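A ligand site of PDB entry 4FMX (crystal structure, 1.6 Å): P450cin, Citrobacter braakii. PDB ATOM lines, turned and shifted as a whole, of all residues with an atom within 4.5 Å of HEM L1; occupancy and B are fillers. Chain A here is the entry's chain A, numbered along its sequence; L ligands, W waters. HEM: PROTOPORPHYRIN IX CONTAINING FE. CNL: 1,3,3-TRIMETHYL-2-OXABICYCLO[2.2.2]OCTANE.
A ring nitrogen (NE2) of His 92 lies within hydrogen-bond range of an oxygen (O1D) of HEM L1 (2.6 Å).
The side-chain sulfur (SG) of Cys 341 is bound to an iron atom (FE) of HEM L1 (2.4 Å).
O1D of HEM L1 is in salt-bridge range of NH1 of Arg 96, 2.8 Å away.
The side-chain amide nitrogen of Asn 67 is in hydrogen-bond range of an oxygen (O2A) of HEM L1 (3.0 Å).
ND2 of Asn 236 lies within hydrogen-bond range of O of CNL L2 (2.8 Å).
ND1 of His 339 lies within hydrogen-bond range of O2D of HEM L1, 2.7 Å away.
O2D of HEM L1 is in hydrogen-bond range of N of Ala 85 (3.4 Å).
NH1 of Arg 283 lies within salt-bridge range of O2A of HEM L1, at 2.9 Å.
The backbone carbonyl oxygen (O) of Leu 334 sits at hydrogen-bond distance from the backbone NH (N) of Cys 341 (2.9 Å).
O of Gly 232 is in hydrogen-bond range of OG1 of Thr 237 (2.8 Å).
The backbone carbonyl oxygen (O) of Ala 85 sits at hydrogen-bond distance from the side-chain amide nitrogen (ND2) of Asn 67 (2.8 Å).
NE2 of His 92 lies close to O of Ile 338 (3.4 Å).
A ring nitrogen (ND1) of His 339 lies close to a ring nitrogen (NE2) of His 92 (3.4 Å).
NE2 of His 339 lies close to OD1 of Asn 67, 3.2 Å away.
The side-chain amide oxygen (OD1) of Asn 67 sits close to the guanidinium group (NE) of Arg 283.
The backbone carbonyl oxygen (O) of Leu 273 lies within hydrogen-bond range of the side-chain hydroxyl (OG) of Ser 333 (2.6 Å).
The backbone carbonyl oxygen of Met 84 lies close to an oxygen (O2D) of HEM L1, 3.3 Å away.
A nitrogen (NB) of HEM L1 sits close to the side-chain amide nitrogen of Asn 236, 3.4 Å away.
O of Ile 338 lies close to O1D of HEM L1, 3.4 Å away.
Residues that only touch HEM L1: Val 70 (3.5 Å), Phe 103 (3.7 Å), Leu 150 (3.8 Å), Ile 228 (3.96 Å), Leu 229 (3.8 Å), Gly 232 (3.4 Å), Gly 233 (3.8 Å), Thr 237 (3.5 Å), Phe 240 (3.7 Å), Pro 278 (3.8 Å), Val 281 (3.7 Å), Phe 306 (3.6 Å), Ser 333 (3.4 Å), Leu 334 (3.6 Å), Gly 335 (3.5 Å), Leu 342 (3.8 Å), Gly 343 (3.98 Å) and Ile 347 (3.5 Å).
The nearest printed residue that does not touch HEM L1 is Arg 340 (4.1 Å).
Water W3 lies within hydrogen-bond range of O of Ser 333 (2.7 Å) and N of Ala 279 (2.9 Å).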
ATOM      1  N   ILE A  59      13.632 -27.714  -5.326  1.00  0.00           N
ATOM      2  CA  ILE A  59      13.199 -27.308  -3.989  1.00  0.00           C
ATOM      3  C   ILE A  59      11.715 -27.585  -3.740  1.00  0.00           C
ATOM      4  O   ILE A  59      11.301 -27.851  -2.612  1.00  0.00           O
ATOM      5  CB  ILE A  59      13.579 -25.806  -3.761  1.00  0.00           C
ATOM      6  CG1 ILE A  59      14.302 -25.628  -2.417  1.00  0.00           C
ATOM      7  CG2 ILE A  59      12.370 -24.924  -3.824  1.00  0.00           C
ATOM      8  CD1 ILE A  59      14.931 -24.258  -2.242  1.00  0.00           C
ATOM      9  N   ASN A  67      15.690 -33.242   2.665  1.00  0.00           N
ATOM     10  CA  ASN A  67      16.577 -32.364   3.431  1.00  0.00           C
ATOM     11  C   ASN A  67      17.538 -33.092   4.367  1.00  0.00           C
ATOM     12  O   ASN A  67      18.286 -32.469   5.106  1.00  0.00           O
ATOM     13  CB  ASN A  67      15.775 -31.304   4.197  1.00  0.00           C
ATOM     14  CG  ASN A  67      15.602 -30.040   3.375  1.00  0.00           C
ATOM     15  OD1 ASN A  67      15.106 -30.081   2.262  1.00  0.00           O
ATOM     16  ND2 ASN A  67      16.045 -28.911   3.928  1.00  0.00           N
ATOM     17  N   VAL A  70      20.760 -31.553   3.583  1.00  0.00           N
ATOM     18  CA  VAL A  70      20.777 -30.088   3.628  1.00  0.00           C
ATOM     19  C   VAL A  70      22.197 -29.518   3.721  1.00  0.00           C
ATOM     20  O   VAL A  70      22.506 -28.510   3.064  1.00  0.00           O
ATOM     21  CB  VAL A  70      19.869 -29.533   4.770  1.00  0.00           C
ATOM     22  CG1 VAL A  70      20.391 -29.925   6.122  1.00  0.00           C
ATOM     23  CG2 VAL A  70      19.733 -28.013   4.649  1.00  0.00           C
ATOM     24  N   MET A  84      14.580 -28.935  12.050  1.00  0.00           N
ATOM     25  CA  MET A  84      13.812 -28.353  10.934  1.00  0.00           C
ATOM     26  C   MET A  84      14.538 -28.485   9.600  1.00  0.00           C
ATOM     27  O   MET A  84      14.051 -29.155   8.683  1.00  0.00           O
ATOM     28  CB  MET A  84      13.438 -26.894  11.213  1.00  0.00           C
ATOM     29  CG  MET A  84      12.407 -26.739  12.357  1.00  0.00           C
ATOM     30  SD  MET A  84      12.164 -25.036  12.833  1.00  0.00           S
ATOM     31  CE  MET A  84      13.658 -24.742  13.769  1.00  0.00           C
ATOM     32  N   ALA A  85      15.702 -27.874   9.500  1.00  0.00           N
ATOM     33  CA  ALA A  85      16.460 -27.837   8.260  1.00  0.00           C
ATOM     34  C   ALA A  85      16.866 -29.217   7.740  1.00  0.00           C
ATOM     35  O   ALA A  85      16.998 -29.418   6.538  1.00  0.00           O
ATOM     36  CB  ALA A  85      17.683 -26.980   8.442  1.00  0.00           C
ATOM     37  N   HIS A  92       9.405 -32.400  10.104  1.00  0.00           N
ATOM     38  CA  HIS A  92       9.826 -31.015   9.960  1.00  0.00           C
ATOM     39  C   HIS A  92       8.752 -30.016  10.385  1.00  0.00           C
ATOM     40  O   HIS A  92       9.029 -29.091  11.169  1.00  0.00           O
ATOM     41  CB  HIS A  92      10.225 -30.759   8.496  1.00  0.00           C
ATOM     42  CG  HIS A  92      10.105 -29.333   8.072  1.00  0.00           C
ATOM     43  ND1 HIS A  92       8.999 -28.837   7.423  1.00  0.00           N
ATOM     44  CD2 HIS A  92      10.977 -28.293   8.170  1.00  0.00           C
ATOM     45  CE1 HIS A  92       9.178 -27.551   7.160  1.00  0.00           C
ATOM     46  NE2 HIS A  92      10.374 -27.208   7.599  1.00  0.00           N
ATOM     47  N   ARG A  96       8.649 -27.021  13.304  1.00  0.00           N
ATOM     48  CA  ARG A  96       8.575 -25.621  12.915  1.00  0.00           C
ATOM     49  C   ARG A  96       7.355 -24.943  13.535  1.00  0.00           C
ATOM     50  O   ARG A  96       7.401 -23.767  13.882  1.00  0.00           O
ATOM     51  CB  ARG A  96       8.549 -25.455  11.389  1.00  0.00           C
ATOM     52  CG  ARG A  96       8.568 -23.986  10.992  1.00  0.00           C
ATOM     53  CD  ARG A  96       9.033 -23.780   9.586  1.00  0.00           C
ATOM     54  NE  ARG A  96       8.908 -22.372   9.227  1.00  0.00           N
ATOM     55  CZ  ARG A  96       9.572 -21.779   8.246  1.00  0.00           C
ATOM     56  NH1 ARG A  96      10.428 -22.459   7.492  1.00  0.00           N
ATOM     57  NH2 ARG A  96       9.377 -20.494   8.006  1.00  0.00           N
ATOM     58  N   PHE A 103       8.907 -16.097  15.483  1.00  0.00           N
ATOM     59  CA  PHE A 103       9.649 -15.616  14.327  1.00  0.00           C
ATOM     60  C   PHE A 103       8.761 -14.908  13.281  1.00  0.00           C
ATOM     61  O   PHE A 103       9.252 -14.502  12.225  1.00  0.00           O
ATOM     62  CB  PHE A 103      10.413 -16.772  13.690  1.00  0.00           C
ATOM     63  CG  PHE A 103      11.669 -17.133  14.442  1.00  0.00           C
ATOM     64  CD1 PHE A 103      12.821 -16.401  14.265  1.00  0.00           C
ATOM     65  CD2 PHE A 103      11.675 -18.198  15.326  1.00  0.00           C
ATOM     66  CE1 PHE A 103      13.983 -16.733  14.964  1.00  0.00           C
ATOM     67  CE2 PHE A 103      12.823 -18.540  16.028  1.00  0.00           C
ATOM     68  CZ  PHE A 103      13.980 -17.807  15.842  1.00  0.00           C
ATOM     69  N   LEU A 150      18.021 -14.514  21.892  1.00  0.00           N
ATOM     70  CA  LEU A 150      17.046 -15.519  21.457  1.00  0.00           C
ATOM     71  C   LEU A 150      17.166 -16.798  22.248  1.00  0.00           C
ATOM     72  O   LEU A 150      16.167 -17.457  22.534  1.00  0.00           O
ATOM     73  CB  LEU A 150      17.230 -15.870  19.979  1.00  0.00           C
ATOM     74  CG  LEU A 150      16.879 -14.816  18.948  1.00  0.00           C
ATOM     75  CD1 LEU A 150      17.141 -15.359  17.542  1.00  0.00           C
ATOM     76  CD2 LEU A 150      15.434 -14.404  19.070  1.00  0.00           C
ATOM     77  N   ILE A 228      20.667 -24.958  15.613  1.00  0.00           N
ATOM     78  CA  ILE A 228      20.282 -24.369  14.339  1.00  0.00           C
ATOM     79  C   ILE A 228      20.141 -22.836  14.449  1.00  0.00           C
ATOM     80  O   ILE A 228      20.505 -22.093  13.551  1.00  0.00           O
ATOM     81  CB  ILE A 228      18.978 -25.008  13.794  1.00  0.00           C
ATOM     82  CG1 ILE A 228      18.875 -24.822  12.284  1.00  0.00           C
ATOM     83  CG2 ILE A 228      17.742 -24.474  14.518  1.00  0.00           C
ATOM     84  CD1 ILE A 228      19.815 -25.704  11.511  1.00  0.00           C
ATOM     85  N   LEU A 229      19.611 -22.373  15.583  1.00  0.00           N
ATOM     86  CA  LEU A 229      19.480 -20.929  15.760  1.00  0.00           C
ATOM     87  C   LEU A 229      20.885 -20.295  15.909  1.00  0.00           C
ATOM     88  O   LEU A 229      21.157 -19.222  15.388  1.00  0.00           O
ATOM     89  CB  LEU A 229      18.595 -20.604  16.962  1.00  0.00           C
ATOM     90  CG  LEU A 229      17.209 -21.281  16.912  1.00  0.00           C
ATOM     91  CD1 LEU A 229      16.435 -20.971  18.201  1.00  0.00           C
ATOM     92  CD2 LEU A 229      16.400 -20.870  15.719  1.00  0.00           C
ATOM     93  N   GLY A 232      22.316 -19.971  12.299  1.00  0.00           N
ATOM     94  CA  GLY A 232      21.717 -18.890  11.520  1.00  0.00           C
ATOM     95  C   GLY A 232      22.249 -17.510  11.884  1.00  0.00           C
ATOM     96  O   GLY A 232      22.436 -16.653  11.010  1.00  0.00           O
ATOM     97  N   GLY A 233      22.468 -17.269  13.169  1.00  0.00           N
ATOM     98  CA  GLY A 233      22.991 -15.998  13.609  1.00  0.00           C
ATOM     99  C   GLY A 233      24.507 -15.831  13.426  1.00  0.00           C
ATOM    100  O   GLY A 233      24.973 -14.901  12.783  1.00  0.00           O
ATOM    101  N   ASN A 236      25.485 -17.594   9.192  1.00  0.00           N
ATOM    102  CA  ASN A 236      24.791 -17.011   8.050  1.00  0.00           C
ATOM    103  C   ASN A 236      24.697 -15.485   8.117  1.00  0.00           C
ATOM    104  O   ASN A 236      25.097 -14.790   7.189  1.00  0.00           O
ATOM    105  CB  ASN A 236      23.375 -17.566   7.914  1.00  0.00           C
ATOM    106  CG  ASN A 236      23.346 -19.093   7.797  1.00  0.00           C
ATOM    107  OD1 ASN A 236      24.240 -19.800   8.253  1.00  0.00           O
ATOM    108  ND2 ASN A 236      22.284 -19.602   7.199  1.00  0.00           N
ATOM    109  N   THR A 237      24.181 -14.958   9.219  1.00  0.00           N
ATOM    110  CA  THR A 237      23.913 -13.517   9.291  1.00  0.00           C
ATOM    111  C   THR A 237      25.215 -12.715   9.327  1.00  0.00           C
ATOM    112  O   THR A 237      25.325 -11.670   8.660  1.00  0.00           O
ATOM    113  CB  THR A 237      23.059 -13.157  10.526  1.00  0.00           C
ATOM    114  OG1 THR A 237      21.844 -13.918  10.547  1.00  0.00           O
ATOM    115  CG2 THR A 237      22.694 -11.695  10.450  1.00  0.00           C
ATOM    116  N   PHE A 240      26.794 -12.624   5.862  1.00  0.00           N
ATOM    117  CA  PHE A 240      26.040 -11.713   5.020  1.00  0.00           C
ATOM    118  C   PHE A 240      26.371 -10.261   5.343  1.00  0.00           C
ATOM    119  O   PHE A 240      26.708  -9.478   4.457  1.00  0.00           O
ATOM    120  CB  PHE A 240      24.533 -11.945   5.156  1.00  0.00           C
ATOM    121  CG  PHE A 240      23.707 -10.899   4.462  1.00  0.00           C
ATOM    122  CD1 PHE A 240      22.863 -10.083   5.178  1.00  0.00           C
ATOM    123  CD2 PHE A 240      23.802 -10.715   3.091  1.00  0.00           C
ATOM    124  CE1 PHE A 240      22.111  -9.116   4.543  1.00  0.00           C
ATOM    125  CE2 PHE A 240      23.067  -9.750   2.465  1.00  0.00           C
ATOM    126  CZ  PHE A 240      22.214  -8.953   3.174  1.00  0.00           C
ATOM    127  N   LEU A 273      20.621  -9.008  -0.291  1.00  0.00           N
ATOM    128  CA  LEU A 273      20.426 -10.440  -0.064  1.00  0.00           C
ATOM    129  C   LEU A 273      20.564 -11.224  -1.358  1.00  0.00           C
ATOM    130  O   LEU A 273      21.203 -12.276  -1.404  1.00  0.00           O
ATOM    131  CB  LEU A 273      19.074 -10.718   0.577  1.00  0.00           C
ATOM    132  CG  LEU A 273      19.037 -10.457   2.087  1.00  0.00           C
ATOM    133  CD1 LEU A 273      17.584 -10.360   2.568  1.00  0.00           C
ATOM    134  CD2 LEU A 273      19.831 -11.522   2.854  1.00  0.00           C
ATOM    135  N   PRO A 278      24.725 -15.517   1.403  1.00  0.00           N
ATOM    136  CA  PRO A 278      25.905 -16.391   1.496  1.00  0.00           C
ATOM    137  C   PRO A 278      25.646 -17.888   1.363  1.00  0.00           C
ATOM    138  O   PRO A 278      26.601 -18.662   1.183  1.00  0.00           O
ATOM    139  CB  PRO A 278      26.428 -16.084   2.909  1.00  0.00           C
ATOM    140  CG  PRO A 278      25.181 -15.736   3.678  1.00  0.00           C
ATOM    141  CD  PRO A 278      24.321 -14.988   2.711  1.00  0.00           C
ATOM    142  N   ALA A 279      24.386 -18.305   1.462  1.00  0.00           N
ATOM    143  CA  ALA A 279      24.074 -19.727   1.632  1.00  0.00           C
ATOM    144  C   ALA A 279      23.873 -20.524   0.359  1.00  0.00           C
ATOM    145  O   ALA A 279      23.379 -20.012  -0.661  1.00  0.00           O
ATOM    146  CB  ALA A 279      22.860 -19.886   2.496  1.00  0.00           C
ATOM    147  N   VAL A 281      22.468 -24.814  -0.227  1.00  0.00           N
ATOM    148  CA  VAL A 281      21.987 -26.023   0.472  1.00  0.00           C
ATOM    149  C   VAL A 281      22.065 -27.245  -0.436  1.00  0.00           C
ATOM    150  O   VAL A 281      22.097 -27.139  -1.654  1.00  0.00           O
ATOM    151  CB  VAL A 281      20.544 -25.904   1.019  1.00  0.00           C
ATOM    152  CG1 VAL A 281      20.445 -24.796   2.043  1.00  0.00           C
ATOM    153  CG2 VAL A 281      19.514 -25.707  -0.093  1.00  0.00           C
ATOM    154  N   ARG A 283      20.476 -31.368  -1.276  1.00  0.00           N
ATOM    155  CA  ARG A 283      19.332 -32.261  -1.181  1.00  0.00           C
ATOM    156  C   ARG A 283      19.799 -33.681  -1.472  1.00  0.00           C
ATOM    157  O   ARG A 283      20.575 -33.896  -2.388  1.00  0.00           O
ATOM    158  CB  ARG A 283      18.244 -31.895  -2.182  1.00  0.00           C
ATOM    159  CG  ARG A 283      17.597 -30.540  -1.970  1.00  0.00           C
ATOM    160  CD  ARG A 283      16.697 -30.551  -0.742  1.00  0.00           C
ATOM    161  NE  ARG A 283      15.880 -29.338  -0.563  1.00  0.00           N
ATOM    162  CZ  ARG A 283      16.215 -28.278   0.165  1.00  0.00           C
ATOM    163  NH1 ARG A 283      17.380 -28.208   0.790  1.00  0.00           N
ATOM    164  NH2 ARG A 283      15.358 -27.260   0.300  1.00  0.00           N
ATOM    165  N   PHE A 306      22.449 -21.320  -4.926  1.00  0.00           N
ATOM    166  CA  PHE A 306      21.570 -20.164  -4.929  1.00  0.00           C
ATOM    167  C   PHE A 306      22.236 -18.891  -5.535  1.00  0.00           C
ATOM    168  O   PHE A 306      21.583 -18.151  -6.241  1.00  0.00           O
ATOM    169  CB  PHE A 306      21.052 -19.855  -3.524  1.00  0.00           C
ATOM    170  CG  PHE A 306      20.127 -20.897  -2.930  1.00  0.00           C
ATOM    171  CD1 PHE A 306      20.187 -21.183  -1.584  1.00  0.00           C
ATOM    172  CD2 PHE A 306      19.147 -21.510  -3.689  1.00  0.00           C
ATOM    173  CE1 PHE A 306      19.330 -22.094  -1.006  1.00  0.00           C
ATOM    174  CE2 PHE A 306      18.290 -22.431  -3.113  1.00  0.00           C
ATOM    175  CZ  PHE A 306      18.378 -22.717  -1.773  1.00  0.00           C
ATOM    176  N   LEU A 332      16.627 -16.309  -4.221  1.00  0.00           N
ATOM    177  CA  LEU A 332      16.600 -17.593  -3.518  1.00  0.00           C
ATOM    178  C   LEU A 332      17.550 -17.617  -2.318  1.00  0.00           C
ATOM    179  O   LEU A 332      17.811 -18.679  -1.772  1.00  0.00           O
ATOM    180  CB  LEU A 332      16.972 -18.728  -4.476  1.00  0.00           C
ATOM    181  CG  LEU A 332      15.888 -19.095  -5.493  1.00  0.00           C
ATOM    182  CD1 LEU A 332      16.448 -19.952  -6.627  1.00  0.00           C
ATOM    183  CD2 LEU A 332      14.766 -19.812  -4.784  1.00  0.00           C
ATOM    184  N   SER A 333      18.072 -16.460  -1.937  1.00  0.00           N
ATOM    185  CA  SER A 333      18.989 -16.383  -0.804  1.00  0.00           C
ATOM    186  C   SER A 333      18.450 -16.853   0.543  1.00  0.00           C
ATOM    187  O   SER A 333      19.248 -17.184   1.411  1.00  0.00           O
ATOM    188  CB  SER A 333      19.550 -14.976  -0.665  1.00  0.00           C
ATOM    189  OG  SER A 333      20.202 -14.626  -1.888  1.00  0.00           O
ATOM    190  N   LEU A 334      17.126 -16.862   0.704  1.00  0.00           N
ATOM    191  CA  LEU A 334      16.496 -17.344   1.926  1.00  0.00           C
ATOM    192  C   LEU A 334      15.673 -18.602   1.625  1.00  0.00           C
ATOM    193  O   LEU A 334      14.843 -19.026   2.421  1.00  0.00           O
ATOM    194  CB  LEU A 334      15.614 -16.254   2.556  1.00  0.00           C
ATOM    195  CG  LEU A 334      16.346 -14.992   3.014  1.00  0.00           C
ATOM    196  CD1 LEU A 334      15.385 -13.850   3.310  1.00  0.00           C
ATOM    197  CD2 LEU A 334      17.221 -15.298   4.233  1.00  0.00           C
ATOM    198  N   GLY A 335      15.924 -19.217   0.485  1.00  0.00           N
ATOM    199  CA  GLY A 335      15.232 -20.432   0.126  1.00  0.00           C
ATOM    200  C   GLY A 335      13.837 -20.135  -0.399  1.00  0.00           C
ATOM    201  O   GLY A 335      13.529 -19.009  -0.791  1.00  0.00           O
ATOM    202  N   ILE A 338       8.811 -25.098   1.658  1.00  0.00           N
ATOM    203  CA  ILE A 338       8.551 -25.509   3.036  1.00  0.00           C
ATOM    204  C   ILE A 338       9.694 -25.208   3.999  1.00  0.00           C
ATOM    205  O   ILE A 338       9.458 -25.023   5.196  1.00  0.00           O
ATOM    206  CB  ILE A 338       8.086 -26.984   3.180  1.00  0.00           C
ATOM    207  CG1 ILE A 338       9.204 -27.938   2.786  1.00  0.00           C
ATOM    208  CG2 ILE A 338       6.832 -27.238   2.356  1.00  0.00           C
ATOM    209  CD1 ILE A 338       8.959 -29.376   3.239  1.00  0.00           C
ATOM    210  N   HIS A 339      10.927 -25.133   3.487  1.00  0.00           N
ATOM    211  CA  HIS A 339      12.080 -24.850   4.349  1.00  0.00           C
ATOM    212  C   HIS A 339      12.545 -23.399   4.319  1.00  0.00           C
ATOM    213  O   HIS A 339      13.629 -23.098   4.804  1.00  0.00           O
ATOM    214  CB  HIS A 339      13.257 -25.738   3.985  1.00  0.00           C
ATOM    215  CG  HIS A 339      13.023 -27.195   4.256  1.00  0.00           C
ATOM    216  ND1 HIS A 339      13.078 -27.734   5.527  1.00  0.00           N
ATOM    217  CD2 HIS A 339      12.718 -28.214   3.423  1.00  0.00           C
ATOM    218  CE1 HIS A 339      12.826 -29.028   5.455  1.00  0.00           C
ATOM    219  NE2 HIS A 339      12.607 -29.352   4.196  1.00  0.00           N
ATOM    220  N   ARG A 340      11.736 -22.501   3.771  1.00  0.00           N
ATOM    221  CA  ARG A 340      12.152 -21.107   3.636  1.00  0.00           C
ATOM    222  C   ARG A 340      12.588 -20.570   4.998  1.00  0.00           C
ATOM    223  O   ARG A 340      11.934 -20.835   6.019  1.00  0.00           O
ATOM    224  CB  ARG A 340      11.028 -20.267   3.059  1.00  0.00           C
ATOM    225  CG  ARG A 340      11.444 -18.821   2.754  1.00  0.00           C
ATOM    226  CD  ARG A 340      10.313 -17.998   2.148  1.00  0.00           C
ATOM    227  NE  ARG A 340      10.742 -16.626   1.867  1.00  0.00           N
ATOM    228  CZ  ARG A 340      10.684 -15.622   2.741  1.00  0.00           C
ATOM    229  NH1 ARG A 340      10.200 -15.816   3.962  1.00  0.00           N
ATOM    230  NH2 ARG A 340      11.111 -14.424   2.394  1.00  0.00           N
ATOM    231  N   CYS A 341      13.671 -19.808   5.005  1.00  0.00           N
ATOM    232  CA  CYS A 341      14.302 -19.330   6.221  1.00  0.00           C
ATOM    233  C   CYS A 341      13.339 -18.879   7.319  1.00  0.00           C
ATOM    234  O   CYS A 341      12.553 -17.936   7.138  1.00  0.00           O
ATOM    235  CB  CYS A 341      15.233 -18.161   5.900  1.00  0.00           C
ATOM    236  SG  CYS A 341      16.160 -17.586   7.323  1.00  0.00           S
ATOM    237  N   LEU A 342      13.437 -19.537   8.475  1.00  0.00           N
ATOM    238  CA  LEU A 342      12.640 -19.191   9.649  1.00  0.00           C
ATOM    239  C   LEU A 342      12.979 -17.786  10.111  1.00  0.00           C
ATOM    240  O   LEU A 342      12.128 -17.081  10.660  1.00  0.00           O
ATOM    241  CB  LEU A 342      12.925 -20.202  10.762  1.00  0.00           C
ATOM    242  CG  LEU A 342      12.207 -19.979  12.099  1.00  0.00           C
ATOM    243  CD1 LEU A 342      10.716 -20.215  11.928  1.00  0.00           C
ATOM    244  CD2 LEU A 342      12.774 -20.890  13.144  1.00  0.00           C
ATOM    245  N   GLY A 343      14.223 -17.375   9.897  1.00  0.00           N
ATOM    246  CA  GLY A 343      14.684 -16.084  10.349  1.00  0.00           C
ATOM    247  C   GLY A 343      14.540 -14.968   9.330  1.00  0.00           C
ATOM    248  O   GLY A 343      15.089 -13.901   9.531  1.00  0.00           O
ATOM    249  N   ILE A 347      16.093 -11.210  10.029  1.00  0.00           N
ATOM    250  CA  ILE A 347      17.352 -10.749   9.480  1.00  0.00           C
ATOM    251  C   ILE A 347      17.130  -9.541   8.553  1.00  0.00           C
ATOM    252  O   ILE A 347      18.005  -8.724   8.407  1.00  0.00           O
ATOM    253  CB  ILE A 347      18.167 -11.873   8.819  1.00  0.00           C
ATOM    254  CG1 ILE A 347      17.479 -12.403   7.553  1.00  0.00           C
ATOM    255  CG2 ILE A 347      18.409 -13.010   9.824  1.00  0.00           C
ATOM    256  CD1 ILE A 347      17.967 -11.721   6.291  1.00  0.00           C
HETATM  257  CHA HEM L   1      16.493 -22.045   6.453  1.00  0.00           C
HETATM  258  CHB HEM L   1      19.483 -18.670   4.627  1.00  0.00           C
HETATM  259  CHC HEM L   1      19.659 -16.516   8.999  1.00  0.00           C
HETATM  260  CHD HEM L   1      17.071 -20.152  10.966  1.00  0.00           C
HETATM  261  C1A HEM L   1      17.237 -21.315   5.557  1.00  0.00           C
HETATM  262  C2A HEM L   1      17.390 -21.579   4.128  1.00  0.00           C
HETATM  263  C3A HEM L   1      18.228 -20.639   3.647  1.00  0.00           C
HETATM  264  C4A HEM L   1      18.619 -19.754   4.727  1.00  0.00           C
HETATM  265  CMA HEM L   1      18.717 -20.488   2.191  1.00  0.00           C
HETATM  266  CAA HEM L   1      16.714 -22.707   3.297  1.00  0.00           C
HETATM  267  CBA HEM L   1      17.143 -24.104   3.733  1.00  0.00           C
HETATM  268  CGA HEM L   1      16.806 -25.156   2.690  1.00  0.00           C
HETATM  269  O1A HEM L   1      16.170 -24.880   1.655  1.00  0.00           O
HETATM  270  O2A HEM L   1      17.171 -26.336   2.936  1.00  0.00           O
HETATM  271  C1B HEM L   1      19.754 -17.763   5.638  1.00  0.00           C
HETATM  272  C2B HEM L   1      20.431 -16.497   5.493  1.00  0.00           C
HETATM  273  C3B HEM L   1      20.502 -15.919   6.691  1.00  0.00           C
HETATM  274  C4B HEM L   1      19.817 -16.769   7.644  1.00  0.00           C
HETATM  275  CMB HEM L   1      20.993 -15.998   4.151  1.00  0.00           C
HETATM  276  CAB HEM L   1      21.108 -14.544   7.086  1.00  0.00           C
HETATM  277  CBB HEM L   1      21.332 -13.548   6.213  1.00  0.00           C
HETATM  278  C1C HEM L   1      18.943 -17.291   9.919  1.00  0.00           C
HETATM  279  C2C HEM L   1      18.692 -16.968  11.308  1.00  0.00           C
HETATM  280  C3C HEM L   1      17.982 -17.960  11.859  1.00  0.00           C
HETATM  281  C4C HEM L   1      17.753 -18.958  10.839  1.00  0.00           C
HETATM  282  CMC HEM L   1      19.172 -15.676  12.005  1.00  0.00           C
HETATM  283  CAC HEM L   1      17.445 -18.109  13.298  1.00  0.00           C
HETATM  284  CBC HEM L   1      17.538 -17.202  14.275  1.00  0.00           C
HETATM  285  C1D HEM L   1      16.732 -21.005   9.943  1.00  0.00           C
HETATM  286  C2D HEM L   1      16.018 -22.244  10.116  1.00  0.00           C
HETATM  287  C3D HEM L   1      15.852 -22.825   8.722  1.00  0.00           C
HETATM  288  C4D HEM L   1      16.462 -21.877   7.816  1.00  0.00           C
HETATM  289  CMD HEM L   1      15.529 -22.882  11.429  1.00  0.00           C
HETATM  290  CAD HEM L   1      15.140 -24.145   8.398  1.00  0.00           C
HETATM  291  CBD HEM L   1      13.658 -23.805   8.211  1.00  0.00           C
HETATM  292  CGD HEM L   1      12.874 -25.042   7.888  1.00  0.00           C
HETATM  293  O1D HEM L   1      11.618 -24.933   7.811  1.00  0.00           O
HETATM  294  O2D HEM L   1      13.506 -26.103   7.674  1.00  0.00           O
HETATM  295  NA  HEM L   1      17.994 -20.209   5.885  1.00  0.00           N
HETATM  296  NB  HEM L   1      19.386 -17.894   6.970  1.00  0.00           N
HETATM  297  NC  HEM L   1      18.347 -18.503   9.675  1.00  0.00           N
HETATM  298  ND  HEM L   1      16.979 -20.826   8.568  1.00  0.00           N
HETATM  299 FE   HEM L   1      17.932 -19.176   7.692  1.00  0.00          FE
HETATM  300  C1  CNL L   2      21.340 -23.164   8.384  1.00  0.00           C
HETATM  301  C2  CNL L   2      20.035 -23.676   7.864  1.00  0.00           C
HETATM  302  C3  CNL L   2      20.169 -24.623   6.749  1.00  0.00           C
HETATM  303  C4  CNL L   2      21.572 -24.645   6.246  1.00  0.00           C
HETATM  304  C5  CNL L   2      22.454 -25.042   7.297  1.00  0.00           C
HETATM  305  C6  CNL L   2      22.312 -24.285   8.574  1.00  0.00           C
HETATM  306  C7  CNL L   2      21.151 -22.284   9.564  1.00  0.00           C
HETATM  307  C8  CNL L   2      21.877 -23.186   5.936  1.00  0.00           C
HETATM  308  C9  CNL L   2      20.826 -22.592   5.050  1.00  0.00           C
HETATM  309  C10 CNL L   2      23.194 -22.971   5.243  1.00  0.00           C
HETATM  310  O   CNL L   2      21.884 -22.392   7.281  1.00  0.00           O
HETATM  311  O   HOH W   1      13.948 -23.441   1.156  1.00  0.00           O
HETATM  312  O   HOH W   2      20.703 -12.818  13.065  1.00  0.00           O
HETATM  313  O   HOH W   3      21.890 -16.887   0.950  1.00  0.00           O
HETATM  314  O   HOH W   4      20.039 -16.613  15.848  1.00  0.00           O
